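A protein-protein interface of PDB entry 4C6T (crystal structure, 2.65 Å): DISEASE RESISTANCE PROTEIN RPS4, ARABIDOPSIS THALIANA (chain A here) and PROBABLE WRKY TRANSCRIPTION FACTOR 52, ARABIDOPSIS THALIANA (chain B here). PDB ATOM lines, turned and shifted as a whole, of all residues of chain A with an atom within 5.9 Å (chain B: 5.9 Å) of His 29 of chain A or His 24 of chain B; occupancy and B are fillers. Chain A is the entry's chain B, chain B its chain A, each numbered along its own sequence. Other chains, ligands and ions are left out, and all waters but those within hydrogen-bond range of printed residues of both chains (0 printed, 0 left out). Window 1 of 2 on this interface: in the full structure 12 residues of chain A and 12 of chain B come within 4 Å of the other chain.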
ATOM      1  N   ARG A  23     -14.398  -8.980 -25.969  1.00  0.00           N
ATOM      2  CA  ARG A  23     -15.230  -8.866 -24.770  1.00  0.00           C
ATOM      3  C   ARG A  23     -16.244 -10.024 -24.701  1.00  0.00           C
ATOM      4  O   ARG A  23     -16.463 -10.629 -23.643  1.00  0.00           O
ATOM      5  CB  ARG A  23     -15.955  -7.511 -24.748  1.00  0.00           C
ATOM      6  CG  ARG A  23     -17.050  -7.387 -23.692  1.00  0.00           C
ATOM      7  CD  ARG A  23     -16.456  -7.389 -22.275  1.00  0.00           C
ATOM      8  NE  ARG A  23     -17.492  -7.422 -21.239  1.00  0.00           N
ATOM      9  CZ  ARG A  23     -18.013  -8.548 -20.751  1.00  0.00           C
ATOM     10  NH1 ARG A  23     -17.579  -9.723 -21.210  1.00  0.00           N
ATOM     11  NH2 ARG A  23     -18.945  -8.510 -19.800  1.00  0.00           N
ATOM     12  N   ARG A  24     -16.850 -10.335 -25.837  1.00  0.00           N
ATOM     13  CA  ARG A  24     -17.803 -11.418 -25.877  1.00  0.00           C
ATOM     14  C   ARG A  24     -17.165 -12.802 -25.740  1.00  0.00           C
ATOM     15  O   ARG A  24     -17.832 -13.743 -25.328  1.00  0.00           O
ATOM     16  CB  ARG A  24     -18.636 -11.314 -27.144  1.00  0.00           C
ATOM     17  CG  ARG A  24     -19.837 -10.410 -26.937  1.00  0.00           C
ATOM     18  CD  ARG A  24     -20.801 -10.446 -28.096  1.00  0.00           C
ATOM     19  NE  ARG A  24     -20.119 -10.229 -29.367  1.00  0.00           N
ATOM     20  CZ  ARG A  24     -20.035  -9.046 -29.970  1.00  0.00           C
ATOM     21  NH1 ARG A  24     -20.597  -7.978 -29.421  1.00  0.00           N
ATOM     22  NH2 ARG A  24     -19.395  -8.928 -31.127  1.00  0.00           N
ATOM     23  N   ARG A  25     -15.889 -12.940 -26.087  1.00  0.00           N
ATOM     24  CA  ARG A  25     -15.226 -14.256 -26.029  1.00  0.00           C
ATOM     25  C   ARG A  25     -14.280 -14.403 -24.832  1.00  0.00           C
ATOM     26  O   ARG A  25     -14.716 -14.473 -23.679  1.00  0.00           O
ATOM     27  CB  ARG A  25     -14.470 -14.513 -27.331  1.00  0.00           C
ATOM     28  CG  ARG A  25     -15.388 -14.594 -28.516  1.00  0.00           C
ATOM     29  CD  ARG A  25     -14.673 -15.076 -29.743  1.00  0.00           C
ATOM     30  NE  ARG A  25     -15.611 -15.799 -30.604  1.00  0.00           N
ATOM     31  CZ  ARG A  25     -15.396 -16.101 -31.883  1.00  0.00           C
ATOM     32  NH1 ARG A  25     -14.274 -15.701 -32.470  1.00  0.00           N
ATOM     33  NH2 ARG A  25     -16.315 -16.774 -32.577  1.00  0.00           N
ATOM     34  N   PHE A  26     -12.987 -14.399 -25.106  1.00  0.00           N
ATOM     35  CA  PHE A  26     -11.998 -14.679 -24.080  1.00  0.00           C
ATOM     36  C   PHE A  26     -12.198 -13.871 -22.810  1.00  0.00           C
ATOM     37  O   PHE A  26     -12.163 -14.448 -21.709  1.00  0.00           O
ATOM     38  CB  PHE A  26     -10.579 -14.443 -24.596  1.00  0.00           C
ATOM     39  CG  PHE A  26      -9.531 -14.741 -23.566  1.00  0.00           C
ATOM     40  CD1 PHE A  26      -9.189 -16.059 -23.269  1.00  0.00           C
ATOM     41  CD2 PHE A  26      -8.913 -13.715 -22.856  1.00  0.00           C
ATOM     42  CE1 PHE A  26      -8.249 -16.332 -22.301  1.00  0.00           C
ATOM     43  CE2 PHE A  26      -7.953 -13.997 -21.885  1.00  0.00           C
ATOM     44  CZ  PHE A  26      -7.630 -15.293 -21.607  1.00  0.00           C
ATOM     45  N   VAL A  27     -12.415 -12.561 -22.943  1.00  0.00           N
ATOM     46  CA  VAL A  27     -12.565 -11.720 -21.757  1.00  0.00           C
ATOM     47  C   VAL A  27     -13.802 -12.155 -20.957  1.00  0.00           C
ATOM     48  O   VAL A  27     -13.757 -12.139 -19.721  1.00  0.00           O
ATOM     49  CB  VAL A  27     -12.630 -10.220 -22.102  1.00  0.00           C
ATOM     50  CG1 VAL A  27     -13.121  -9.415 -20.924  1.00  0.00           C
ATOM     51  CG2 VAL A  27     -11.226  -9.694 -22.494  1.00  0.00           C
ATOM     52  N   SER A  28     -14.883 -12.575 -21.622  1.00  0.00           N
ATOM     53  CA  SER A  28     -16.073 -12.978 -20.858  1.00  0.00           C
ATOM     54  C   SER A  28     -15.764 -14.173 -19.896  1.00  0.00           C
ATOM     55  O   SER A  28     -16.300 -14.257 -18.792  1.00  0.00           O
ATOM     56  CB  SER A  28     -17.255 -13.311 -21.785  1.00  0.00           C
ATOM     57  OG  SER A  28     -17.185 -14.614 -22.337  1.00  0.00           O
ATOM     58  N   HIS A  29     -14.890 -15.081 -20.308  1.00  0.00           N
ATOM     59  CA  HIS A  29     -14.511 -16.174 -19.433  1.00  0.00           C
ATOM     60  C   HIS A  29     -13.609 -15.719 -18.298  1.00  0.00           C
ATOM     61  O   HIS A  29     -13.790 -16.128 -17.133  1.00  0.00           O
ATOM     62  CB  HIS A  29     -13.835 -17.279 -20.242  1.00  0.00           C
ATOM     63  CG  HIS A  29     -14.736 -17.865 -21.272  1.00  0.00           C
ATOM     64  ND1 HIS A  29     -14.440 -17.853 -22.618  1.00  0.00           N
ATOM     65  CD2 HIS A  29     -15.982 -18.385 -21.169  1.00  0.00           C
ATOM     66  CE1 HIS A  29     -15.441 -18.382 -23.295  1.00  0.00           C
ATOM     67  NE2 HIS A  29     -16.393 -18.703 -22.443  1.00  0.00           N
ATOM     68  N   LEU A  30     -12.641 -14.870 -18.637  1.00  0.00           N
ATOM     69  CA  LEU A  30     -11.770 -14.303 -17.627  1.00  0.00           C
ATOM     70  C   LEU A  30     -12.615 -13.563 -16.572  1.00  0.00           C
ATOM     71  O   LEU A  30     -12.410 -13.732 -15.363  1.00  0.00           O
ATOM     72  CB  LEU A  30     -10.744 -13.397 -18.277  1.00  0.00           C
ATOM     73  CG  LEU A  30      -9.783 -12.658 -17.354  1.00  0.00           C
ATOM     74  CD1 LEU A  30      -9.108 -13.639 -16.430  1.00  0.00           C
ATOM     75  CD2 LEU A  30      -8.741 -11.919 -18.199  1.00  0.00           C
ATOM     76  N   VAL A  31     -13.587 -12.783 -17.031  1.00  0.00           N
ATOM     77  CA  VAL A  31     -14.439 -12.067 -16.104  1.00  0.00           C
ATOM     78  C   VAL A  31     -15.274 -13.040 -15.239  1.00  0.00           C
ATOM     79  O   VAL A  31     -15.406 -12.863 -14.028  1.00  0.00           O
ATOM     80  CB  VAL A  31     -15.324 -11.047 -16.867  1.00  0.00           C
ATOM     81  CG1 VAL A  31     -16.455 -10.480 -15.990  1.00  0.00           C
ATOM     82  CG2 VAL A  31     -14.428  -9.921 -17.377  1.00  0.00           C
ATOM     83  N   THR A  32     -15.830 -14.070 -15.852  1.00  0.00           N
ATOM     84  CA  THR A  32     -16.590 -15.011 -15.068  1.00  0.00           C
ATOM     85  C   THR A  32     -15.713 -15.690 -13.988  1.00  0.00           C
ATOM     86  O   THR A  32     -16.169 -15.870 -12.869  1.00  0.00           O
ATOM     87  CB  THR A  32     -17.257 -16.056 -15.961  1.00  0.00           C
ATOM     88  OG1 THR A  32     -18.337 -15.428 -16.665  1.00  0.00           O
ATOM     89  CG2 THR A  32     -17.826 -17.230 -15.112  1.00  0.00           C
ATOM     90  N   ALA A  33     -14.459 -16.014 -14.309  1.00  0.00           N
ATOM     91  CA  ALA A  33     -13.598 -16.682 -13.347  1.00  0.00           C
ATOM     92  C   ALA A  33     -13.185 -15.739 -12.191  1.00  0.00           C
ATOM     93  O   ALA A  33     -13.099 -16.150 -11.035  1.00  0.00           O
ATOM     94  CB  ALA A  33     -12.366 -17.251 -14.039  1.00  0.00           C
ATOM     95  N   LEU A  34     -12.931 -14.474 -12.500  1.00  0.00           N
ATOM     96  CA  LEU A  34     -12.598 -13.549 -11.445  1.00  0.00           C
ATOM     97  C   LEU A  34     -13.787 -13.354 -10.497  1.00  0.00           C
ATOM     98  O   LEU A  34     -13.626 -13.355  -9.266  1.00  0.00           O
ATOM     99  CB  LEU A  34     -12.140 -12.207 -12.011  1.00  0.00           C
ATOM    100  CG  LEU A  34     -10.856 -12.233 -12.867  1.00  0.00           C
ATOM    101  CD1 LEU A  34     -10.690 -10.932 -13.697  1.00  0.00           C
ATOM    102  CD2 LEU A  34      -9.611 -12.523 -12.029  1.00  0.00           C
ATOM    103  N   GLU A 155      -7.076 -22.012 -23.804  1.00  0.00           N
ATOM    104  CA  GLU A 155      -7.499 -20.740 -23.218  1.00  0.00           C
ATOM    105  C   GLU A 155      -7.962 -20.891 -21.786  1.00  0.00           C
ATOM    106  O   GLU A 155      -7.675 -20.050 -20.944  1.00  0.00           O
ATOM    107  CB  GLU A 155      -8.601 -20.096 -24.060  1.00  0.00           C
ATOM    108  CG  GLU A 155      -8.048 -19.240 -25.179  1.00  0.00           C
ATOM    109  CD  GLU A 155      -9.114 -18.511 -25.976  1.00  0.00           C
ATOM    110  OE1 GLU A 155     -10.323 -18.527 -25.605  1.00  0.00           O
ATOM    111  OE2 GLU A 155      -8.725 -17.898 -26.987  1.00  0.00           O
ATOM    112  N   SER A 156      -8.642 -21.989 -21.502  1.00  0.00           N
ATOM    113  CA  SER A 156      -9.195 -22.156 -20.181  1.00  0.00           C
ATOM    114  C   SER A 156      -8.060 -22.232 -19.162  1.00  0.00           C
ATOM    115  O   SER A 156      -8.206 -21.802 -18.023  1.00  0.00           O
ATOM    116  CB  SER A 156     -10.107 -23.395 -20.129  1.00  0.00           C
ATOM    117  OG  SER A 156      -9.378 -24.583 -20.352  1.00  0.00           O
ATOM    118  N   VAL A 159      -6.751 -18.631 -18.660  1.00  0.00           N
ATOM    119  CA  VAL A 159      -7.661 -17.962 -17.733  1.00  0.00           C
ATOM    120  C   VAL A 159      -7.314 -18.330 -16.295  1.00  0.00           C
ATOM    121  O   VAL A 159      -7.122 -17.436 -15.454  1.00  0.00           O
ATOM    122  CB  VAL A 159      -9.138 -18.338 -17.967  1.00  0.00           C
ATOM    123  CG1 VAL A 159      -9.998 -17.902 -16.786  1.00  0.00           C
ATOM    124  CG2 VAL A 159      -9.664 -17.749 -19.263  1.00  0.00           C
ATOM    125  N   TYR B  19      -9.034 -25.265 -28.769  1.00  0.00           N
ATOM    126  CA  TYR B  19      -8.251 -24.638 -27.724  1.00  0.00           C
ATOM    127  C   TYR B  19      -8.896 -23.361 -27.218  1.00  0.00           C
ATOM    128  O   TYR B  19      -8.426 -22.789 -26.243  1.00  0.00           O
ATOM    129  CB  TYR B  19      -6.841 -24.351 -28.227  1.00  0.00           C
ATOM    130  CG  TYR B  19      -6.150 -25.598 -28.720  1.00  0.00           C
ATOM    131  CD1 TYR B  19      -5.833 -26.628 -27.842  1.00  0.00           C
ATOM    132  CD2 TYR B  19      -5.841 -25.755 -30.067  1.00  0.00           C
ATOM    133  CE1 TYR B  19      -5.223 -27.776 -28.290  1.00  0.00           C
ATOM    134  CE2 TYR B  19      -5.229 -26.896 -30.529  1.00  0.00           C
ATOM    135  CZ  TYR B  19      -4.919 -27.910 -29.637  1.00  0.00           C
ATOM    136  OH  TYR B  19      -4.301 -29.065 -30.087  1.00  0.00           O
ATOM    137  N   SER B  20      -9.978 -22.913 -27.847  1.00  0.00           N
ATOM    138  CA  SER B  20     -10.643 -21.710 -27.351  1.00  0.00           C
ATOM    139  C   SER B  20     -11.982 -22.079 -26.724  1.00  0.00           C
ATOM    140  O   SER B  20     -12.024 -22.519 -25.564  1.00  0.00           O
ATOM    141  CB  SER B  20     -10.858 -20.662 -28.449  1.00  0.00           C
ATOM    142  OG  SER B  20     -11.446 -21.215 -29.610  1.00  0.00           O
ATOM    143  N   PHE B  21     -13.068 -21.920 -27.487  1.00  0.00           N
ATOM    144  CA  PHE B  21     -14.413 -22.084 -26.923  1.00  0.00           C
ATOM    145  C   PHE B  21     -14.608 -23.426 -26.208  1.00  0.00           C
ATOM    146  O   PHE B  21     -15.121 -23.456 -25.093  1.00  0.00           O
ATOM    147  CB  PHE B  21     -15.484 -21.923 -28.011  1.00  0.00           C
ATOM    148  CG  PHE B  21     -16.886 -22.193 -27.528  1.00  0.00           C
ATOM    149  CD1 PHE B  21     -17.524 -21.302 -26.673  1.00  0.00           C
ATOM    150  CD2 PHE B  21     -17.580 -23.321 -27.952  1.00  0.00           C
ATOM    151  CE1 PHE B  21     -18.819 -21.533 -26.238  1.00  0.00           C
ATOM    152  CE2 PHE B  21     -18.884 -23.565 -27.522  1.00  0.00           C
ATOM    153  CZ  PHE B  21     -19.497 -22.677 -26.655  1.00  0.00           C
ATOM    154  N   VAL B  22     -14.183 -24.523 -26.828  1.00  0.00           N
ATOM    155  CA  VAL B  22     -14.419 -25.832 -26.231  1.00  0.00           C
ATOM    156  C   VAL B  22     -13.641 -26.005 -24.925  1.00  0.00           C
ATOM    157  O   VAL B  22     -14.137 -26.662 -24.006  1.00  0.00           O
ATOM    158  CB  VAL B  22     -14.068 -26.989 -27.204  1.00  0.00           C
ATOM    159  CG1 VAL B  22     -14.057 -28.325 -26.496  1.00  0.00           C
ATOM    160  CG2 VAL B  22     -15.063 -27.036 -28.355  1.00  0.00           C
ATOM    161  N   SER B  23     -12.438 -25.435 -24.822  1.00  0.00           N
ATOM    162  CA  SER B  23     -11.674 -25.585 -23.580  1.00  0.00           C
ATOM    163  C   SER B  23     -12.425 -24.961 -22.412  1.00  0.00           C
ATOM    164  O   SER B  23     -12.409 -25.488 -21.292  1.00  0.00           O
ATOM    165  CB  SER B  23     -10.264 -24.986 -23.689  1.00  0.00           C
ATOM    166  OG  SER B  23     -10.281 -23.582 -23.581  1.00  0.00           O
ATOM    167  N   HIS B  24     -13.108 -23.856 -22.672  1.00  0.00           N
ATOM    168  CA  HIS B  24     -13.908 -23.220 -21.633  1.00  0.00           C
ATOM    169  C   HIS B  24     -15.080 -24.092 -21.271  1.00  0.00           C
ATOM    170  O   HIS B  24     -15.416 -24.229 -20.083  1.00  0.00           O
ATOM    171  CB  HIS B  24     -14.398 -21.838 -22.082  1.00  0.00           C
ATOM    172  CG  HIS B  24     -13.277 -20.893 -22.337  1.00  0.00           C
ATOM    173  ND1 HIS B  24     -12.438 -20.455 -21.327  1.00  0.00           N
ATOM    174  CD2 HIS B  24     -12.793 -20.376 -23.493  1.00  0.00           C
ATOM    175  CE1 HIS B  24     -11.513 -19.663 -21.848  1.00  0.00           C
ATOM    176  NE2 HIS B  24     -11.698 -19.603 -23.159  1.00  0.00           N
ATOM    177  N   LEU B  25     -15.665 -24.707 -22.297  1.00  0.00           N
ATOM    178  CA  LEU B  25     -16.797 -25.588 -22.104  1.00  0.00           C
ATOM    179  C   LEU B  25     -16.399 -26.782 -21.232  1.00  0.00           C
ATOM    180  O   LEU B  25     -17.100 -27.110 -20.240  1.00  0.00           O
ATOM    181  CB  LEU B  25     -17.326 -26.058 -23.445  1.00  0.00           C
ATOM    182  CG  LEU B  25     -18.538 -26.982 -23.317  1.00  0.00           C
ATOM    183  CD1 LEU B  25     -19.602 -26.307 -22.426  1.00  0.00           C
ATOM    184  CD2 LEU B  25     -19.119 -27.350 -24.699  1.00  0.00           C
ATOM    185  N   SER B  26     -15.260 -27.388 -21.568  1.00  0.00           N
ATOM    186  CA  SER B  26     -14.750 -28.537 -20.818  1.00  0.00           C
ATOM    187  C   SER B  26     -14.369 -28.152 -19.393  1.00  0.00           C
ATOM    188  O   SER B  26     -14.582 -28.923 -18.453  1.00  0.00           O
ATOM    189  CB  SER B  26     -13.572 -29.168 -21.540  1.00  0.00           C
ATOM    190  OG  SER B  26     -12.882 -30.020 -20.660  1.00  0.00           O
ATOM    191  N   GLU B  27     -13.796 -26.965 -19.226  1.00  0.00           N
ATOM    192  CA  GLU B  27     -13.465 -26.508 -17.881  1.00  0.00           C
ATOM    193  C   GLU B  27     -14.732 -26.306 -17.028  1.00  0.00           C
ATOM    194  O   GLU B  27     -14.748 -26.626 -15.830  1.00  0.00           O
ATOM    195  CB  GLU B  27     -12.657 -25.211 -17.946  1.00  0.00           C
ATOM    196  CG  GLU B  27     -12.295 -24.606 -16.611  1.00  0.00           C
ATOM    197  CD  GLU B  27     -11.235 -25.432 -15.883  1.00  0.00           C
ATOM    198  OE1 GLU B  27     -10.598 -26.297 -16.552  1.00  0.00           O
ATOM    199  OE2 GLU B  27     -11.005 -25.195 -14.660  1.00  0.00           O
ATOM    200  N   ALA B  28     -15.786 -25.761 -17.634  1.00  0.00           N
ATOM    201  CA  ALA B  28     -17.004 -25.480 -16.880  1.00  0.00           C
ATOM    202  C   ALA B  28     -17.683 -26.751 -16.337  1.00  0.00           C
ATOM    203  O   ALA B  28     -18.108 -26.790 -15.177  1.00  0.00           O
ATOM    204  CB  ALA B  28     -17.960 -24.718 -17.723  1.00  0.00           C
ATOM    205  N   LEU B  29     -17.760 -27.780 -17.177  1.00  0.00           N
ATOM    206  CA  LEU B  29     -18.298 -29.063 -16.764  1.00  0.00           C
ATOM    207  C   LEU B  29     -17.452 -29.634 -15.629  1.00  0.00           C
ATOM    208  O   LEU B  29     -17.970 -30.197 -14.659  1.00  0.00           O
ATOM    209  CB  LEU B  29     -18.322 -30.034 -17.940  1.00  0.00           C
ATOM    210  CG  LEU B  29     -19.280 -29.740 -19.098  1.00  0.00           C
ATOM    211  CD1 LEU B  29     -18.959 -30.612 -20.304  1.00  0.00           C
ATOM    212  CD2 LEU B  29     -20.729 -29.933 -18.684  1.00  0.00           C
ATOM    213  N   ARG B  31     -15.636 -28.062 -13.411  1.00  0.00           N
ATOM    214  CA  ARG B  31     -15.875 -27.329 -12.156  1.00  0.00           C
ATOM    215  C   ARG B  31     -17.144 -27.807 -11.458  1.00  0.00           C
ATOM    216  O   ARG B  31     -17.268 -27.738 -10.239  1.00  0.00           O
ATOM    217  CB  ARG B  31     -15.987 -25.819 -12.417  1.00  0.00           C
ATOM    218  CG  ARG B  31     -14.686 -25.100 -12.761  1.00  0.00           C
ATOM    219  CD  ARG B  31     -15.005 -23.722 -13.337  1.00  0.00           C
ATOM    220  NE  ARG B  31     -13.824 -22.971 -13.763  1.00  0.00           N
ATOM    221  CZ  ARG B  31     -13.874 -21.840 -14.470  1.00  0.00           C
ATOM    222  NH1 ARG B  31     -15.051 -21.363 -14.866  1.00  0.00           N
ATOM    223  NH2 ARG B  31     -12.748 -21.203 -14.800  1.00  0.00           N
ATOM    224  N   ASP B 129     -19.820 -15.710 -24.913  1.00  0.00           N
ATOM    225  CA  ASP B 129     -19.539 -17.131 -25.009  1.00  0.00           C
ATOM    226  C   ASP B 129     -19.634 -17.766 -23.628  1.00  0.00           C
ATOM    227  O   ASP B 129     -19.938 -18.962 -23.503  1.00  0.00           O
ATOM    228  CB  ASP B 129     -18.162 -17.379 -25.599  1.00  0.00           C
ATOM    229  CG  ASP B 129     -18.160 -17.341 -27.095  1.00  0.00           C
ATOM    230  OD1 ASP B 129     -19.231 -17.088 -27.689  1.00  0.00           O
ATOM    231  OD2 ASP B 129     -17.072 -17.550 -27.677  1.00  0.00           O
ATOM    232  N   SER B 130     -19.375 -16.956 -22.598  1.00  0.00           N
ATOM    233  CA  SER B 130     -19.472 -17.415 -21.221  1.00  0.00           C
ATOM    234  C   SER B 130     -20.917 -17.771 -20.862  1.00  0.00           C
ATOM    235  O   SER B 130     -21.181 -18.806 -20.265  1.00  0.00           O
ATOM    236  CB  SER B 130     -18.923 -16.346 -20.278  1.00  0.00           C
ATOM    237  OG  SER B 130     -19.189 -16.644 -18.925  1.00  0.00           O
ATOM    238  N   ILE B 131     -21.850 -16.911 -21.237  1.00  0.00           N
ATOM    239  CA  ILE B 131     -23.261 -17.190 -21.049  1.00  0.00           C
ATOM    240  C   ILE B 131     -23.641 -18.430 -21.824  1.00  0.00           C
ATOM    241  O   ILE B 131     -24.369 -19.282 -21.327  1.00  0.00           O
ATOM    242  CB  ILE B 131     -24.137 -15.990 -21.473  1.00  0.00           C
ATOM    243  CG1 ILE B 131     -24.188 -14.994 -20.327  1.00  0.00           C
ATOM    244  CG2 ILE B 131     -25.558 -16.424 -21.817  1.00  0.00           C
ATOM    245  CD1 ILE B 131     -24.795 -15.581 -19.058  1.00  0.00           C
ATOM    246  N   VAL B 133     -21.799 -20.963 -22.593  1.00  0.00           N
ATOM    247  CA  VAL B 133     -21.265 -22.110 -21.889  1.00  0.00           C
ATOM    248  C   VAL B 133     -22.177 -22.438 -20.711  1.00  0.00           C
ATOM    249  O   VAL B 133     -22.491 -23.608 -20.453  1.00  0.00           O
ATOM    250  CB  VAL B 133     -19.819 -21.872 -21.416  1.00  0.00           C
ATOM    251  CG1 VAL B 133     -19.406 -22.927 -20.373  1.00  0.00           C
ATOM    252  CG2 VAL B 133     -18.862 -21.904 -22.616  1.00  0.00           C
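Of the 15 printed residues of chain A, 8 touch a printed residue of chain B.
Hydrophobic or aromatic side chains of chain A within 4 Å of the printed part of chain B: His 29 and Val 159.
Asp 129 of chain B touches Ser 28 of chain A (N to OG, 3.8 Å).
NE2 of His 29 of chain A touches C of Asp 129 of chain B, at 3.6 Å.
OE1 of Glu 155 of chain A touches CB of Ser 20 of chain B, 3.6 Å away.
OG of Ser 23 of chain B touches N of Glu 155 of chain A (3.6 Å).
His 24 of chain B touches Ser 156 of chain A.
Ser 156 of chain A touches Glu 27 of chain B.
CG2 of Val 159 of chain A touches CE1 of His 24 of chain B (3.7 Å).
The backbone NH (N) of Glu 155 of chain A lies within hydrogen-bond range of the backbone carbonyl oxygen (O) of Tyr 19 of chain B (2.9 Å).
N of Ser 156 of chain A sits at hydrogen-bond distance from OG of Ser 23 of chain B.
NE2 of His 24 of chain B lies close to ND1 of His 29 of chain A, at 3.3 Å.
A ring nitrogen (NE2) of His 24 of chain B is in hydrogen-bond range of the side-chain carboxylate (OE1) of Glu 155 of chain A (3.0 Å).
The backbone carbonyl oxygen (O) of Arg 24 of chain A lies within hydrogen-bond range of the backbone NH (N) of Asp 129 of chain B.
NE of Arg 25 of chain A lies within salt-bridge range of OD2 of Asp 129 of chain B.
The backbone NH (N) of Ser 130 of chain B lies close to the side-chain hydroxyl (OG) of Ser 28 of chain A (3.2 Å).
A ring nitrogen (NE2) of His 29 of chain A is in hydrogen-bond range of the backbone NH (N) of Ser 130 of chain B (3.5 Å).
The side-chain hydroxyl (OG) of Ser 130 of chain B is in hydrogen-bond range of the side-chain hydroxyl (OG1) of Thr 32 of chain A, at 2.7 Å.
The backbone carbonyl oxygen of Tyr 19 of chain B lies within hydrogen-bond range of the side-chain hydroxyl of Ser 23 of chain B.
The backbone carbonyl oxygen (O) of Ser 20 of chain B sits at hydrogen-bond distance from the side-chain hydroxyl (OG) of Ser 23 of chain B (2.8 Å).
The guanidinium group (NE) of Arg 31 of chain B lies within salt-bridge range of the side-chain carboxylate (OE2) of Glu 27 of chain B (3.7 Å).
The backbone NH (N) of Ser 28 of chain A sits at hydrogen-bond distance from the backbone carbonyl oxygen (O) of Arg 23 of chain A (3.2 Å).
OG of Ser 28 of chain A is in hydrogen-bond range of O of Arg 24 of chain A (3.2 Å).
The backbone carbonyl oxygen (O) of Ser 28 of chain A sits at hydrogen-bond distance from the side-chain hydroxyl (OG1) of Thr 32 of chain A (3.2 Å).
Of the printed residues of chain B, His 29 of chain A touches His 24, Asp 129 and Ser 130.
Leu 34 of chain A touches none of the printed residues of chain B.
Of the printed residues of chain B, Glu 155 of chain A touches Tyr 19 (2.9 Å), Ser 20 (3.6 Å), Ser 23 (3.6 Å) and His 24 (3.0 Å).
His 24 of chain B touches four residues of chain A.
Printed residues of chain A within 4 Å of Ser 130 of chain B: Ser 28, His 29 and Thr 32.
The nearest residue of chain B that does not touch His 29 of chain A is Val 133 of chain B (4.05 Å).
The nearest residue of chain A that does not touch His 24 of chain B is Phe 26 of chain A (4.3 Å).
The nearest printed residue of chain B that does not touch Thr 32 of chain A is Arg 31 of chain B (5.0 Å).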
